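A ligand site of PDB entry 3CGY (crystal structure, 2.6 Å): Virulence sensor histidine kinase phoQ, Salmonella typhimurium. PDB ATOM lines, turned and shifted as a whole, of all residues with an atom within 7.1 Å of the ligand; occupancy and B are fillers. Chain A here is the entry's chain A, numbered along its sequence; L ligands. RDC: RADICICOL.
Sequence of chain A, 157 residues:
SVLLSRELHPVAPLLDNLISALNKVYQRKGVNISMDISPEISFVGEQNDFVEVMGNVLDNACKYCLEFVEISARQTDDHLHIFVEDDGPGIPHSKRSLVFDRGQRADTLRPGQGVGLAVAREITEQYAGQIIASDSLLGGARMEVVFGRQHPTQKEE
The backbone NH (N) of Asp 86 lies within hydrogen-bond range of the backbone carbonyl oxygen (O) of Ala 141 (3.1 Å).
O of Asp 86 sits at hydrogen-bond distance from N of Gly 140.
The side-chain carboxylate (OD1) of Asp 86 sits at hydrogen-bond distance from the backbone NH (N) of Gly 88 (3.0 Å).
An oxygen (O5) of the ligand lies close to the backbone carbonyl oxygen (O) of Gly 90, at 3.3 Å.
Tyr 64 touches the ligand (CB to O4, 3.1 Å).
Pro 89 touches the ligand.
Ile 91 touches the ligand.
Val 115 touches the ligand (O to C18, 2.8 Å).
Leu 117 touches the ligand (CG to C17, 3.6 Å).
Ala 141 touches the ligand.
Hydrophobic or aromatic side chains within 4 Å of the ligand: Tyr 64, Ile 91, Val 115, Leu 117 and Ala 141.
Within 4 Å of the ligand: Asn 60, Tyr 64, Asp 86, Pro 89, Gly 90, Ile 91, Val 115, Leu 117, Arg 121 and Ala 141.
The nearest printed residue that does not touch the ligand is Met 143 (4.2 Å).
An oxygen (O6) of the ligand sits at hydrogen-bond distance from the guanidinium group (NH2) of Arg 121, at 2.6 Å.
An oxygen (O3) of the ligand lies within hydrogen-bond range of the side-chain amide oxygen (OD1) of Asn 60, at 2.8 Å.
An oxygen (O4) of the ligand sits at hydrogen-bond distance from the side-chain carboxylate (OD2) of Asp 86 (3.0 Å).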
ATOM      1  N   ASN A  56       3.950  36.357  23.839  1.00  0.00           N
ATOM      2  CA  ASN A  56       2.972  35.836  22.902  1.00  0.00           C
ATOM      3  C   ASN A  56       3.143  34.305  22.730  1.00  0.00           C
ATOM      4  O   ASN A  56       2.193  33.534  22.761  1.00  0.00           O
ATOM      5  CB  ASN A  56       3.179  36.546  21.561  1.00  0.00           C
ATOM      6  CG  ASN A  56       2.091  36.232  20.573  1.00  0.00           C
ATOM      7  OD1 ASN A  56       1.150  35.503  20.891  1.00  0.00           O
ATOM      8  ND2 ASN A  56       2.209  36.777  19.365  1.00  0.00           N
ATOM      9  N   VAL A  57       4.385  33.876  22.543  1.00  0.00           N
ATOM     10  CA  VAL A  57       4.680  32.475  22.359  1.00  0.00           C
ATOM     11  C   VAL A  57       4.495  31.684  23.637  1.00  0.00           C
ATOM     12  O   VAL A  57       3.883  30.626  23.622  1.00  0.00           O
ATOM     13  CB  VAL A  57       6.119  32.297  21.781  1.00  0.00           C
ATOM     14  CG1 VAL A  57       6.542  30.830  21.856  1.00  0.00           C
ATOM     15  CG2 VAL A  57       6.129  32.731  20.326  1.00  0.00           C
ATOM     16  N   ASN A  60       0.695  31.353  24.451  1.00  0.00           N
ATOM     17  CA  ASN A  60       0.114  30.358  23.568  1.00  0.00           C
ATOM     18  C   ASN A  60       0.542  28.928  23.960  1.00  0.00           C
ATOM     19  O   ASN A  60      -0.246  27.986  23.881  1.00  0.00           O
ATOM     20  CB  ASN A  60       0.526  30.698  22.131  1.00  0.00           C
ATOM     21  CG  ASN A  60      -0.586  30.476  21.136  1.00  0.00           C
ATOM     22  OD1 ASN A  60      -0.610  29.464  20.442  1.00  0.00           O
ATOM     23  ND2 ASN A  60      -1.526  31.409  21.068  1.00  0.00           N
ATOM     24  N   ALA A  61       1.784  28.774  24.404  1.00  0.00           N
ATOM     25  CA  ALA A  61       2.267  27.465  24.809  1.00  0.00           C
ATOM     26  C   ALA A  61       1.449  26.952  25.976  1.00  0.00           C
ATOM     27  O   ALA A  61       0.978  25.821  25.964  1.00  0.00           O
ATOM     28  CB  ALA A  61       3.751  27.520  25.196  1.00  0.00           C
ATOM     29  N   LYS A  63      -1.495  27.665  26.875  1.00  0.00           N
ATOM     30  CA  LYS A  63      -2.862  27.354  26.489  1.00  0.00           C
ATOM     31  C   LYS A  63      -3.030  25.974  25.890  1.00  0.00           C
ATOM     32  O   LYS A  63      -3.879  25.197  26.334  1.00  0.00           O
ATOM     33  CB  LYS A  63      -3.382  28.361  25.476  1.00  0.00           C
ATOM     34  CG  LYS A  63      -3.576  29.742  25.994  1.00  0.00           C
ATOM     35  CD  LYS A  63      -4.267  30.544  24.924  1.00  0.00           C
ATOM     36  CE  LYS A  63      -4.545  31.945  25.367  1.00  0.00           C
ATOM     37  NZ  LYS A  63      -5.275  32.676  24.296  1.00  0.00           N
ATOM     38  N   TYR A  64      -2.232  25.654  24.869  1.00  0.00           N
ATOM     39  CA  TYR A  64      -2.328  24.366  24.203  1.00  0.00           C
ATOM     40  C   TYR A  64      -1.701  23.194  24.938  1.00  0.00           C
ATOM     41  O   TYR A  64      -1.969  22.038  24.602  1.00  0.00           O
ATOM     42  CB  TYR A  64      -1.744  24.452  22.791  1.00  0.00           C
ATOM     43  CG  TYR A  64      -2.512  25.397  21.884  1.00  0.00           C
ATOM     44  CD1 TYR A  64      -2.018  26.666  21.583  1.00  0.00           C
ATOM     45  CD2 TYR A  64      -3.749  25.034  21.366  1.00  0.00           C
ATOM     46  CE1 TYR A  64      -2.741  27.546  20.797  1.00  0.00           C
ATOM     47  CE2 TYR A  64      -4.480  25.910  20.586  1.00  0.00           C
ATOM     48  CZ  TYR A  64      -3.972  27.168  20.299  1.00  0.00           C
ATOM     49  OH  TYR A  64      -4.721  28.072  19.561  1.00  0.00           O
ATOM     50  N   CYS A  65      -0.893  23.469  25.943  1.00  0.00           N
ATOM     51  CA  CYS A  65      -0.258  22.388  26.681  1.00  0.00           C
ATOM     52  C   CYS A  65      -1.260  21.643  27.559  1.00  0.00           C
ATOM     53  O   CYS A  65      -2.415  22.052  27.717  1.00  0.00           O
ATOM     54  CB  CYS A  65       0.880  22.934  27.551  1.00  0.00           C
ATOM     55  SG  CYS A  65       0.362  23.509  29.195  1.00  0.00           S
ATOM     56  N   ASP A  86       5.801  21.988  24.327  1.00  0.00           N
ATOM     57  CA  ASP A  86       4.756  21.595  25.249  1.00  0.00           C
ATOM     58  C   ASP A  86       4.260  20.168  25.013  1.00  0.00           C
ATOM     59  O   ASP A  86       4.466  19.595  23.961  1.00  0.00           O
ATOM     60  CB  ASP A  86       3.578  22.572  25.153  1.00  0.00           C
ATOM     61  CG  ASP A  86       2.873  22.545  23.804  1.00  0.00           C
ATOM     62  OD1 ASP A  86       2.216  21.522  23.470  1.00  0.00           O
ATOM     63  OD2 ASP A  86       2.967  23.551  23.070  1.00  0.00           O
ATOM     64  N   ASP A  87       3.589  19.638  26.019  1.00  0.00           N
ATOM     65  CA  ASP A  87       3.070  18.276  25.982  1.00  0.00           C
ATOM     66  C   ASP A  87       1.577  18.276  25.628  1.00  0.00           C
ATOM     67  O   ASP A  87       0.900  17.282  25.845  1.00  0.00           O
ATOM     68  CB  ASP A  87       3.207  17.660  27.355  1.00  0.00           C
ATOM     69  CG  ASP A  87       2.171  18.198  28.329  1.00  0.00           C
ATOM     70  OD1 ASP A  87       1.616  19.283  28.034  1.00  0.00           O
ATOM     71  OD2 ASP A  87       1.904  17.555  29.364  1.00  0.00           O
ATOM     72  N   GLY A  88       1.046  19.383  25.143  1.00  0.00           N
ATOM     73  CA  GLY A  88      -0.366  19.350  24.834  1.00  0.00           C
ATOM     74  C   GLY A  88      -0.543  18.712  23.473  1.00  0.00           C
ATOM     75  O   GLY A  88       0.452  18.406  22.832  1.00  0.00           O
ATOM     76  N   PRO A  89      -1.782  18.426  23.048  1.00  0.00           N
ATOM     77  CA  PRO A  89      -1.877  17.836  21.720  1.00  0.00           C
ATOM     78  C   PRO A  89      -1.063  18.740  20.781  1.00  0.00           C
ATOM     79  O   PRO A  89      -0.940  19.942  21.043  1.00  0.00           O
ATOM     80  CB  PRO A  89      -3.370  17.844  21.462  1.00  0.00           C
ATOM     81  CG  PRO A  89      -3.894  17.469  22.848  1.00  0.00           C
ATOM     82  CD  PRO A  89      -3.059  18.339  23.776  1.00  0.00           C
ATOM     83  N   GLY A  90      -0.503  18.199  19.706  1.00  0.00           N
ATOM     84  CA  GLY A  90       0.351  18.994  18.842  1.00  0.00           C
ATOM     85  C   GLY A  90      -0.051  19.643  17.526  1.00  0.00           C
ATOM     86  O   GLY A  90      -1.229  19.874  17.232  1.00  0.00           O
ATOM     87  N   ILE A  91       0.973  19.936  16.740  1.00  0.00           N
ATOM     88  CA  ILE A  91       0.839  20.578  15.439  1.00  0.00           C
ATOM     89  C   ILE A  91       1.190  19.616  14.306  1.00  0.00           C
ATOM     90  O   ILE A  91       2.359  19.275  14.112  1.00  0.00           O
ATOM     91  CB  ILE A  91       1.773  21.811  15.332  1.00  0.00           C
ATOM     92  CG1 ILE A  91       3.231  21.361  15.423  1.00  0.00           C
ATOM     93  CG2 ILE A  91       1.504  22.776  16.474  1.00  0.00           C
ATOM     94  CD1 ILE A  91       4.202  22.421  15.062  1.00  0.00           C
ATOM     95  N   PRO A  92       0.177  19.152  13.566  1.00  0.00           N
ATOM     96  CA  PRO A  92       0.435  18.224  12.444  1.00  0.00           C
ATOM     97  C   PRO A  92       0.456  18.956  11.102  1.00  0.00           C
ATOM     98  O   PRO A  92      -0.230  19.968  10.928  1.00  0.00           O
ATOM     99  CB  PRO A  92      -0.735  17.234  12.539  1.00  0.00           C
ATOM    100  CG  PRO A  92      -1.270  17.423  13.960  1.00  0.00           C
ATOM    101  CD  PRO A  92      -1.158  18.909  14.114  1.00  0.00           C
ATOM    102  N   VAL A 115      -1.973  34.178  12.750  1.00  0.00           N
ATOM    103  CA  VAL A 115      -3.024  33.844  13.713  1.00  0.00           C
ATOM    104  C   VAL A 115      -2.463  33.569  15.102  1.00  0.00           C
ATOM    105  O   VAL A 115      -1.653  32.681  15.281  1.00  0.00           O
ATOM    106  CB  VAL A 115      -3.823  32.608  13.249  1.00  0.00           C
ATOM    107  CG1 VAL A 115      -4.604  32.003  14.405  1.00  0.00           C
ATOM    108  CG2 VAL A 115      -4.769  33.008  12.118  1.00  0.00           C
ATOM    109  N   GLY A 116      -2.902  34.345  16.088  1.00  0.00           N
ATOM    110  CA  GLY A 116      -2.377  34.140  17.426  1.00  0.00           C
ATOM    111  C   GLY A 116      -0.953  34.632  17.457  1.00  0.00           C
ATOM    112  O   GLY A 116      -0.673  35.747  17.900  1.00  0.00           O
ATOM    113  N   LEU A 117      -0.028  33.808  16.980  1.00  0.00           N
ATOM    114  CA  LEU A 117       1.371  34.202  16.944  1.00  0.00           C
ATOM    115  C   LEU A 117       1.654  35.289  15.904  1.00  0.00           C
ATOM    116  O   LEU A 117       2.814  35.608  15.635  1.00  0.00           O
ATOM    117  CB  LEU A 117       2.249  32.991  16.693  1.00  0.00           C
ATOM    118  CG  LEU A 117       2.186  31.931  17.788  1.00  0.00           C
ATOM    119  CD1 LEU A 117       3.295  30.931  17.575  1.00  0.00           C
ATOM    120  CD2 LEU A 117       2.334  32.576  19.147  1.00  0.00           C
ATOM    121  N   ALA A 118       0.605  35.867  15.334  1.00  0.00           N
ATOM    122  CA  ALA A 118       0.791  36.909  14.331  1.00  0.00           C
ATOM    123  C   ALA A 118       1.689  38.018  14.890  1.00  0.00           C
ATOM    124  O   ALA A 118       2.623  38.459  14.233  1.00  0.00           O
ATOM    125  CB  ALA A 118      -0.539  37.484  13.923  1.00  0.00           C
ATOM    126  N   ARG A 121       5.042  36.985  15.086  1.00  0.00           N
ATOM    127  CA  ARG A 121       5.540  36.845  13.728  1.00  0.00           C
ATOM    128  C   ARG A 121       5.937  38.206  13.189  1.00  0.00           C
ATOM    129  O   ARG A 121       6.956  38.341  12.516  1.00  0.00           O
ATOM    130  CB  ARG A 121       4.481  36.190  12.825  1.00  0.00           C
ATOM    131  CG  ARG A 121       4.892  34.841  12.234  1.00  0.00           C
ATOM    132  CD  ARG A 121       3.712  34.106  11.590  1.00  0.00           C
ATOM    133  NE  ARG A 121       3.415  32.845  12.287  1.00  0.00           N
ATOM    134  CZ  ARG A 121       4.023  31.680  12.035  1.00  0.00           C
ATOM    135  NH1 ARG A 121       4.949  31.597  11.098  1.00  0.00           N
ATOM    136  NH2 ARG A 121       3.722  30.604  12.746  1.00  0.00           N
ATOM    137  N   ILE A 131       9.444  32.315  12.748  1.00  0.00           N
ATOM    138  CA  ILE A 131       8.910  31.407  13.758  1.00  0.00           C
ATOM    139  C   ILE A 131       8.626  30.067  13.087  1.00  0.00           C
ATOM    140  O   ILE A 131       8.040  29.998  12.013  1.00  0.00           O
ATOM    141  CB  ILE A 131       7.624  31.986  14.394  1.00  0.00           C
ATOM    142  CG1 ILE A 131       8.015  33.094  15.374  1.00  0.00           C
ATOM    143  CG2 ILE A 131       6.831  30.896  15.069  1.00  0.00           C
ATOM    144  CD1 ILE A 131       6.846  33.860  15.964  1.00  0.00           C
ATOM    145  N   ILE A 132       9.078  28.998  13.715  1.00  0.00           N
ATOM    146  CA  ILE A 132       8.878  27.687  13.125  1.00  0.00           C
ATOM    147  C   ILE A 132       8.221  26.679  14.053  1.00  0.00           C
ATOM    148  O   ILE A 132       8.591  26.536  15.236  1.00  0.00           O
ATOM    149  CB  ILE A 132      10.215  27.122  12.622  1.00  0.00           C
ATOM    150  CG1 ILE A 132      10.931  28.164  11.759  1.00  0.00           C
ATOM    151  CG2 ILE A 132       9.957  25.837  11.816  1.00  0.00           C
ATOM    152  CD1 ILE A 132      12.364  27.834  11.458  1.00  0.00           C
ATOM    153  N   ALA A 133       7.240  25.981  13.495  1.00  0.00           N
ATOM    154  CA  ALA A 133       6.490  24.969  14.215  1.00  0.00           C
ATOM    155  C   ALA A 133       7.002  23.583  13.803  1.00  0.00           C
ATOM    156  O   ALA A 133       7.450  23.395  12.677  1.00  0.00           O
ATOM    157  CB  ALA A 133       5.034  25.104  13.874  1.00  0.00           C
ATOM    158  N   GLY A 140       3.563  17.588  22.083  1.00  0.00           N
ATOM    159  CA  GLY A 140       2.918  18.591  21.272  1.00  0.00           C
ATOM    160  C   GLY A 140       3.816  19.391  20.346  1.00  0.00           C
ATOM    161  O   GLY A 140       4.730  18.857  19.708  1.00  0.00           O
ATOM    162  N   ALA A 141       3.515  20.688  20.268  1.00  0.00           N
ATOM    163  CA  ALA A 141       4.264  21.609  19.426  1.00  0.00           C
ATOM    164  C   ALA A 141       5.635  21.942  19.975  1.00  0.00           C
ATOM    165  O   ALA A 141       5.877  21.985  21.179  1.00  0.00           O
ATOM    166  CB  ALA A 141       3.464  22.875  19.237  1.00  0.00           C
ATOM    167  N   ARG A 142       6.567  22.145  19.048  1.00  0.00           N
ATOM    168  CA  ARG A 142       7.921  22.491  19.380  1.00  0.00           C
ATOM    169  C   ARG A 142       8.141  23.776  18.603  1.00  0.00           C
ATOM    170  O   ARG A 142       8.593  23.730  17.463  1.00  0.00           O
ATOM    171  CB  ARG A 142       8.870  21.414  18.897  1.00  0.00           C
ATOM    172  CG  ARG A 142      10.221  21.450  19.538  1.00  0.00           C
ATOM    173  CD  ARG A 142      11.280  21.817  18.550  1.00  0.00           C
ATOM    174  NE  ARG A 142      12.561  21.910  19.228  1.00  0.00           N
ATOM    175  CZ  ARG A 142      13.663  22.414  18.680  1.00  0.00           C
ATOM    176  NH1 ARG A 142      13.635  22.881  17.424  1.00  0.00           N
ATOM    177  NH2 ARG A 142      14.773  22.486  19.413  1.00  0.00           N
ATOM    178  N   MET A 143       7.779  24.903  19.206  1.00  0.00           N
ATOM    179  CA  MET A 143       7.926  26.203  18.569  1.00  0.00           C
ATOM    180  C   MET A 143       9.334  26.742  18.731  1.00  0.00           C
ATOM    181  O   MET A 143       9.837  26.835  19.843  1.00  0.00           O
ATOM    182  CB  MET A 143       6.942  27.223  19.155  1.00  0.00           C
ATOM    183  CG  MET A 143       5.492  26.842  19.068  1.00  0.00           C
ATOM    184  SD  MET A 143       4.912  26.609  17.393  1.00  0.00           S
ATOM    185  CE  MET A 143       4.893  28.236  16.759  1.00  0.00           C
HETATM  186  C1  RDC L   1      -0.741  27.633  17.157  1.00  0.00           C
HETATM  187  C2  RDC L   1      -0.373  26.546  18.166  1.00  0.00           C
HETATM  188  C3  RDC L   1       0.679  26.799  19.145  1.00  0.00           C
HETATM  189  C4  RDC L   1       1.012  25.818  20.066  1.00  0.00           C
HETATM  190  C5  RDC L   1       0.356  24.573  20.111  1.00  0.00           C
HETATM  191  C6  RDC L   1      -0.683  24.272  19.181  1.00  0.00           C
HETATM  192  C7  RDC L   1      -1.067  25.229  18.210  1.00  0.00           C
HETATM  193  C8  RDC L   1      -2.202  24.891  17.197  1.00  0.00           C
HETATM  194  C9  RDC L   1      -1.830  23.934  16.114  1.00  0.00           C
HETATM  195  C10 RDC L   1      -0.966  24.259  14.953  1.00  0.00           C
HETATM  196  C11 RDC L   1      -0.323  25.479  14.675  1.00  0.00           C
HETATM  197  C12 RDC L   1       0.462  25.527  13.406  1.00  0.00           C
HETATM  198  C13 RDC L   1       1.234  26.547  12.848  1.00  0.00           C
HETATM  199  C14 RDC L   1       1.667  28.011  13.231  1.00  0.00           C
HETATM  200  C15 RDC L   1       0.650  29.147  13.683  1.00  0.00           C
HETATM  201  C16 RDC L   1       0.971  29.578  15.143  1.00  0.00           C
HETATM  202  C17 RDC L   1      -0.254  29.931  16.080  1.00  0.00           C
HETATM  203  C18 RDC L   1      -1.638  29.901  15.376  1.00  0.00           C
HETATM  204  O1  RDC L   1      -0.059  28.854  17.101  1.00  0.00           O
HETATM  205  O2  RDC L   1      -1.639  27.375  16.323  1.00  0.00           O
HETATM  206  O3  RDC L   1       1.357  27.942  19.152  1.00  0.00           O
HETATM  207  O4  RDC L   1       0.736  23.698  21.045  1.00  0.00           O
HETATM  208 CL1  RDC L   1      -1.471  22.689  19.284  1.00  0.00          CL
HETATM  209  O5  RDC L   1      -2.316  22.762  16.185  1.00  0.00           O
HETATM  210  O6  RDC L   1       1.531  29.202  12.517  1.00  0.00           O
